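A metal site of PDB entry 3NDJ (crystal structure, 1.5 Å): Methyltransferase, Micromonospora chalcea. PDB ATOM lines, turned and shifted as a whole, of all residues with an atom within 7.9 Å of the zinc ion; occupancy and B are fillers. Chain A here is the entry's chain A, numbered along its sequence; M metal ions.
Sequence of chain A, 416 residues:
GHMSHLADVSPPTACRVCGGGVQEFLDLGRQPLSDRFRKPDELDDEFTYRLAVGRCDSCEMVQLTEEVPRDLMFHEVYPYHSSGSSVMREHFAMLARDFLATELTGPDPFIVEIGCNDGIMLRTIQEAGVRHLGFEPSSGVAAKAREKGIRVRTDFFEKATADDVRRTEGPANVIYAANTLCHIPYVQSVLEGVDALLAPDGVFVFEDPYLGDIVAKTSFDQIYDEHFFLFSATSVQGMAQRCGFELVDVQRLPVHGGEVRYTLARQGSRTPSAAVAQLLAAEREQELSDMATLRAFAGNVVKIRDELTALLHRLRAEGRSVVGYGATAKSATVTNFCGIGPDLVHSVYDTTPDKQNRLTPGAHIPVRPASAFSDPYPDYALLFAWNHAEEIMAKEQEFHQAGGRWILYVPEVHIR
N of Val 17 sits close to SG of Cys 15 (3.3 Å). SG of Cys 56 lies close to N of Ser 58 (3.2 Å). O of Met 61 lies within hydrogen-bond range of N of Cys 56. The backbone carbonyl oxygen (O) of Gly 20 lies within hydrogen-bond range of the backbone NH (N) of Cys 15, at 2.8 Å. The side-chain sulfur of Cys 15 sits close to the side-chain amide nitrogen of Gln 63 (3.4 Å). The backbone NH (N) of Met 61 sits close to the side-chain sulfur (SG) of Cys 59, at 3.5 Å. SG of Cys 18 lies close to N of Gly 20 (3.2 Å).
The zinc ion is bound by the side-chain sulfur (SG) of Cys 59 (2.3 Å), the side-chain sulfur (SG) of Cys 18 (2.3 Å), the side-chain sulfur (SG) of Cys 15 (2.4 Å) and the side-chain sulfur (SG) of Cys 56 (2.4 Å). The zinc ion has four donor atoms within binding distance.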
ATOM      1  N   ALA A  14      12.110   8.624   1.311  1.00  0.00           N
ATOM      2  CA  ALA A  14      12.655   7.848   0.190  1.00  0.00           C
ATOM      3  C   ALA A  14      14.124   7.503   0.472  1.00  0.00           C
ATOM      4  O   ALA A  14      14.927   8.354   0.842  1.00  0.00           O
ATOM      5  CB  ALA A  14      12.625   8.691  -1.103  1.00  0.00           C
ATOM      6  N   CYS A  15      14.497   6.246   0.253  1.00  0.00           N
ATOM      7  CA  CYS A  15      15.879   5.812   0.419  1.00  0.00           C
ATOM      8  C   CYS A  15      16.881   6.685  -0.365  1.00  0.00           C
ATOM      9  O   CYS A  15      16.681   6.952  -1.557  1.00  0.00           O
ATOM     10  CB  CYS A  15      16.065   4.360  -0.054  1.00  0.00           C
ATOM     11  SG  CYS A  15      17.736   3.694  -0.006  1.00  0.00           S
ATOM     12  N   ARG A  16      17.960   7.103   0.306  1.00  0.00           N
ATOM     13  CA  ARG A  16      18.985   7.936  -0.322  1.00  0.00           C
ATOM     14  C   ARG A  16      19.876   7.194  -1.309  1.00  0.00           C
ATOM     15  O   ARG A  16      20.563   7.807  -2.117  1.00  0.00           O
ATOM     16  CB  ARG A  16      19.884   8.619   0.714  1.00  0.00           C
ATOM     17  CG  ARG A  16      19.293   9.906   1.240  1.00  0.00           C
ATOM     18  CD  ARG A  16      19.347  11.028   0.153  1.00  0.00           C
ATOM     19  NE  ARG A  16      19.710  12.361   0.655  1.00  0.00           N
ATOM     20  CZ  ARG A  16      20.342  13.291  -0.057  1.00  0.00           C
ATOM     21  NH1 ARG A  16      20.614  14.462   0.498  1.00  0.00           N
ATOM     22  NH2 ARG A  16      20.699  13.071  -1.327  1.00  0.00           N
ATOM     23  N   VAL A  17      19.840   5.874  -1.280  1.00  0.00           N
ATOM     24  CA  VAL A  17      20.628   5.089  -2.232  1.00  0.00           C
ATOM     25  C   VAL A  17      19.843   4.778  -3.484  1.00  0.00           C
ATOM     26  O   VAL A  17      20.373   5.037  -4.576  1.00  0.00           O
ATOM     27  CB  VAL A  17      21.093   3.781  -1.585  1.00  0.00           C
ATOM     28  CG1 VAL A  17      21.745   2.836  -2.603  1.00  0.00           C
ATOM     29  CG2 VAL A  17      22.063   4.110  -0.466  1.00  0.00           C
ATOM     30  N   CYS A  18      18.634   4.238  -3.323  1.00  0.00           N
ATOM     31  CA  CYS A  18      17.872   3.706  -4.456  1.00  0.00           C
ATOM     32  C   CYS A  18      16.527   4.401  -4.712  1.00  0.00           C
ATOM     33  O   CYS A  18      15.916   4.139  -5.744  1.00  0.00           O
ATOM     34  CB  CYS A  18      17.728   2.182  -4.380  1.00  0.00           C
ATOM     35  SG  CYS A  18      16.479   1.713  -3.186  1.00  0.00           S
ATOM     36  N   GLY A  19      16.064   5.240  -3.794  1.00  0.00           N
ATOM     37  CA  GLY A  19      14.730   5.819  -3.879  1.00  0.00           C
ATOM     38  C   GLY A  19      13.623   4.873  -3.423  1.00  0.00           C
ATOM     39  O   GLY A  19      12.456   5.233  -3.460  1.00  0.00           O
ATOM     40  N   GLY A  20      13.934   3.669  -2.966  1.00  0.00           N
ATOM     41  CA  GLY A  20      12.861   2.853  -2.394  1.00  0.00           C
ATOM     42  C   GLY A  20      12.231   3.328  -1.105  1.00  0.00           C
ATOM     43  O   GLY A  20      12.587   4.364  -0.539  1.00  0.00           O
ATOM     44  N   GLY A  21      11.268   2.571  -0.579  1.00  0.00           N
ATOM     45  CA  GLY A  21      10.574   3.059   0.597  1.00  0.00           C
ATOM     46  C   GLY A  21      11.282   2.637   1.868  1.00  0.00           C
ATOM     47  O   GLY A  21      11.714   1.486   1.947  1.00  0.00           O
ATOM     48  N   VAL A  22      11.398   3.581   2.798  1.00  0.00           N
ATOM     49  CA  VAL A  22      12.074   3.310   4.068  1.00  0.00           C
ATOM     50  C   VAL A  22      11.089   3.120   5.218  1.00  0.00           C
ATOM     51  O   VAL A  22      10.322   4.031   5.523  1.00  0.00           O
ATOM     52  CB  VAL A  22      13.006   4.471   4.477  1.00  0.00           C
ATOM     53  CG1 VAL A  22      13.709   4.166   5.779  1.00  0.00           C
ATOM     54  CG2 VAL A  22      14.063   4.719   3.380  1.00  0.00           C
ATOM     55  N   ARG A  55      14.741   1.106   7.440  1.00  0.00           N
ATOM     56  CA  ARG A  55      15.381   0.251   6.472  1.00  0.00           C
ATOM     57  C   ARG A  55      14.668   0.384   5.128  1.00  0.00           C
ATOM     58  O   ARG A  55      13.435   0.288   5.071  1.00  0.00           O
ATOM     59  CB  ARG A  55      15.345  -1.208   6.976  1.00  0.00           C
ATOM     60  CG  ARG A  55      16.102  -2.114   6.010  1.00  0.00           C
ATOM     61  CD  ARG A  55      15.659  -3.577   6.089  1.00  0.00           C
ATOM     62  NE  ARG A  55      14.419  -3.645   5.332  1.00  0.00           N
ATOM     63  CZ  ARG A  55      13.709  -4.739   5.139  1.00  0.00           C
ATOM     64  NH1 ARG A  55      12.594  -4.658   4.431  1.00  0.00           N
ATOM     65  NH2 ARG A  55      14.133  -5.890   5.650  1.00  0.00           N
ATOM     66  N   CYS A  56      15.461   0.573   4.063  1.00  0.00           N
ATOM     67  CA  CYS A  56      14.872   0.571   2.739  1.00  0.00           C
ATOM     68  C   CYS A  56      14.302  -0.789   2.340  1.00  0.00           C
ATOM     69  O   CYS A  56      14.917  -1.830   2.598  1.00  0.00           O
ATOM     70  CB  CYS A  56      15.886   1.051   1.697  1.00  0.00           C
ATOM     71  SG  CYS A  56      15.272   0.853   0.036  1.00  0.00           S
ATOM     72  N   ASP A  57      13.114  -0.791   1.728  1.00  0.00           N
ATOM     73  CA  ASP A  57      12.485  -2.066   1.325  1.00  0.00           C
ATOM     74  C   ASP A  57      13.135  -2.705   0.095  1.00  0.00           C
ATOM     75  O   ASP A  57      13.018  -3.930  -0.136  1.00  0.00           O
ATOM     76  CB  ASP A  57      11.015  -1.848   0.959  1.00  0.00           C
ATOM     77  CG  ASP A  57      10.156  -1.644   2.165  1.00  0.00           C
ATOM     78  OD1 ASP A  57      10.516  -2.156   3.255  1.00  0.00           O
ATOM     79  OD2 ASP A  57       9.135  -0.955   1.986  1.00  0.00           O
ATOM     80  N   SER A  58      13.818  -1.881  -0.684  1.00  0.00           N
ATOM     81  CA  SER A  58      14.367  -2.335  -1.956  1.00  0.00           C
ATOM     82  C   SER A  58      15.824  -2.794  -1.850  1.00  0.00           C
ATOM     83  O   SER A  58      16.219  -3.827  -2.397  1.00  0.00           O
ATOM     84  CB  SER A  58      14.174  -1.267  -3.027  1.00  0.00           C
ATOM     85  OG  SER A  58      12.795  -0.967  -3.178  1.00  0.00           O
ATOM     86  N   CYS A  59      16.661  -2.055  -1.122  1.00  0.00           N
ATOM     87  CA  CYS A  59      18.095  -2.330  -1.075  1.00  0.00           C
ATOM     88  C   CYS A  59      18.603  -2.703   0.321  1.00  0.00           C
ATOM     89  O   CYS A  59      19.773  -3.051   0.470  1.00  0.00           O
ATOM     90  CB  CYS A  59      18.837  -1.106  -1.677  1.00  0.00           C
ATOM     91  SG  CYS A  59      18.995   0.234  -0.458  1.00  0.00           S
ATOM     92  N   GLU A  60      17.709  -2.643   1.313  1.00  0.00           N
ATOM     93  CA  GLU A  60      18.011  -3.008   2.682  1.00  0.00           C
ATOM     94  C   GLU A  60      18.972  -2.061   3.421  1.00  0.00           C
ATOM     95  O   GLU A  60      19.427  -2.340   4.531  1.00  0.00           O
ATOM     96  CB  GLU A  60      18.507  -4.447   2.765  1.00  0.00           C
ATOM     97  CG  GLU A  60      17.580  -5.416   2.038  1.00  0.00           C
ATOM     98  CD  GLU A  60      18.019  -6.872   2.220  1.00  0.00           C
ATOM     99  OE1 GLU A  60      17.958  -7.366   3.351  1.00  0.00           O
ATOM    100  OE2 GLU A  60      18.419  -7.535   1.239  1.00  0.00           O
ATOM    101  N   MET A  61      19.288  -0.929   2.824  1.00  0.00           N
ATOM    102  CA  MET A  61      20.035   0.101   3.523  1.00  0.00           C
ATOM    103  C   MET A  61      19.314   0.625   4.762  1.00  0.00           C
ATOM    104  O   MET A  61      18.238   1.225   4.645  1.00  0.00           O
ATOM    105  CB  MET A  61      20.420   1.237   2.596  1.00  0.00           C
ATOM    106  CG  MET A  61      21.339   2.285   3.224  1.00  0.00           C
ATOM    107  SD  MET A  61      22.932   1.608   3.704  1.00  0.00           S
ATOM    108  CE  MET A  61      23.802   1.500   2.158  1.00  0.00           C
ATOM    109  N   VAL A  62      19.946   0.483   5.926  1.00  0.00           N
ATOM    110  CA  VAL A  62      19.450   1.106   7.168  1.00  0.00           C
ATOM    111  C   VAL A  62      20.013   2.513   7.213  1.00  0.00           C
ATOM    112  O   VAL A  62      21.197   2.767   7.062  1.00  0.00           O
ATOM    113  CB  VAL A  62      20.038   0.242   8.306  1.00  0.00           C
ATOM    114  CG1 VAL A  62      19.721   0.901   9.632  1.00  0.00           C
ATOM    115  CG2 VAL A  62      19.328  -1.067   8.207  1.00  0.00           C
ATOM    116  N   GLN A  63      19.090   3.438   7.412  1.00  0.00           N
ATOM    117  CA  GLN A  63      19.363   4.881   7.345  1.00  0.00           C
ATOM    118  C   GLN A  63      18.453   5.720   8.246  1.00  0.00           C
ATOM    119  O   GLN A  63      17.345   5.298   8.563  1.00  0.00           O
ATOM    120  CB  GLN A  63      19.273   5.429   5.926  1.00  0.00           C
ATOM    121  CG  GLN A  63      17.870   5.392   5.351  1.00  0.00           C
ATOM    122  CD  GLN A  63      17.987   5.268   3.843  1.00  0.00           C
ATOM    123  OE1 GLN A  63      18.005   6.297   3.143  1.00  0.00           O
ATOM    124  NE2 GLN A  63      18.067   4.044   3.323  1.00  0.00           N
ATOM    125  N   PHE A 229      23.922   6.434   7.826  1.00  0.00           N
ATOM    126  CA  PHE A 229      23.786   5.067   7.342  1.00  0.00           C
ATOM    127  C   PHE A 229      24.395   4.138   8.353  1.00  0.00           C
ATOM    128  O   PHE A 229      25.462   4.431   8.927  1.00  0.00           O
ATOM    129  CB  PHE A 229      24.560   4.875   6.026  1.00  0.00           C
ATOM    130  CG  PHE A 229      23.943   5.575   4.866  1.00  0.00           C
ATOM    131  CD1 PHE A 229      22.708   5.185   4.428  1.00  0.00           C
ATOM    132  CD2 PHE A 229      24.650   6.595   4.257  1.00  0.00           C
ATOM    133  CE1 PHE A 229      22.153   5.863   3.349  1.00  0.00           C
ATOM    134  CE2 PHE A 229      24.134   7.272   3.165  1.00  0.00           C
ATOM    135  CZ  PHE A 229      22.875   6.905   2.713  1.00  0.00           C
ATOM    136  N   SER A 235      23.741  -4.323   2.328  1.00  0.00           N
ATOM    137  CA  SER A 235      23.346  -3.024   1.742  1.00  0.00           C
ATOM    138  C   SER A 235      24.489  -2.420   0.933  1.00  0.00           C
ATOM    139  O   SER A 235      24.256  -1.763  -0.093  1.00  0.00           O
ATOM    140  CB  SER A 235      22.841  -2.107   2.864  1.00  0.00           C
ATOM    141  OG  SER A 235      23.873  -1.828   3.797  1.00  0.00           O
ATOM    142  N   ARG A 242      24.465  -0.856  -7.757  1.00  0.00           N
ATOM    143  CA  ARG A 242      23.538   0.069  -8.397  1.00  0.00           C
ATOM    144  C   ARG A 242      24.330   1.249  -8.949  1.00  0.00           C
ATOM    145  O   ARG A 242      23.717   2.138  -9.538  1.00  0.00           O
ATOM    146  CB  ARG A 242      22.492   0.601  -7.416  1.00  0.00           C
ATOM    147  CG  ARG A 242      21.473  -0.421  -6.952  1.00  0.00           C
ATOM    148  CD  ARG A 242      20.679   0.151  -5.788  1.00  0.00           C
ATOM    149  NE  ARG A 242      19.380  -0.501  -5.703  1.00  0.00           N
ATOM    150  CZ  ARG A 242      19.153  -1.695  -5.169  1.00  0.00           C
ATOM    151  NH1 ARG A 242      20.156  -2.400  -4.655  1.00  0.00           N
ATOM    152  NH2 ARG A 242      17.920  -2.173  -5.166  1.00  0.00           N
HETATM  153 ZN    ZN M   1      17.264   1.600  -1.009  1.00  0.00          ZN
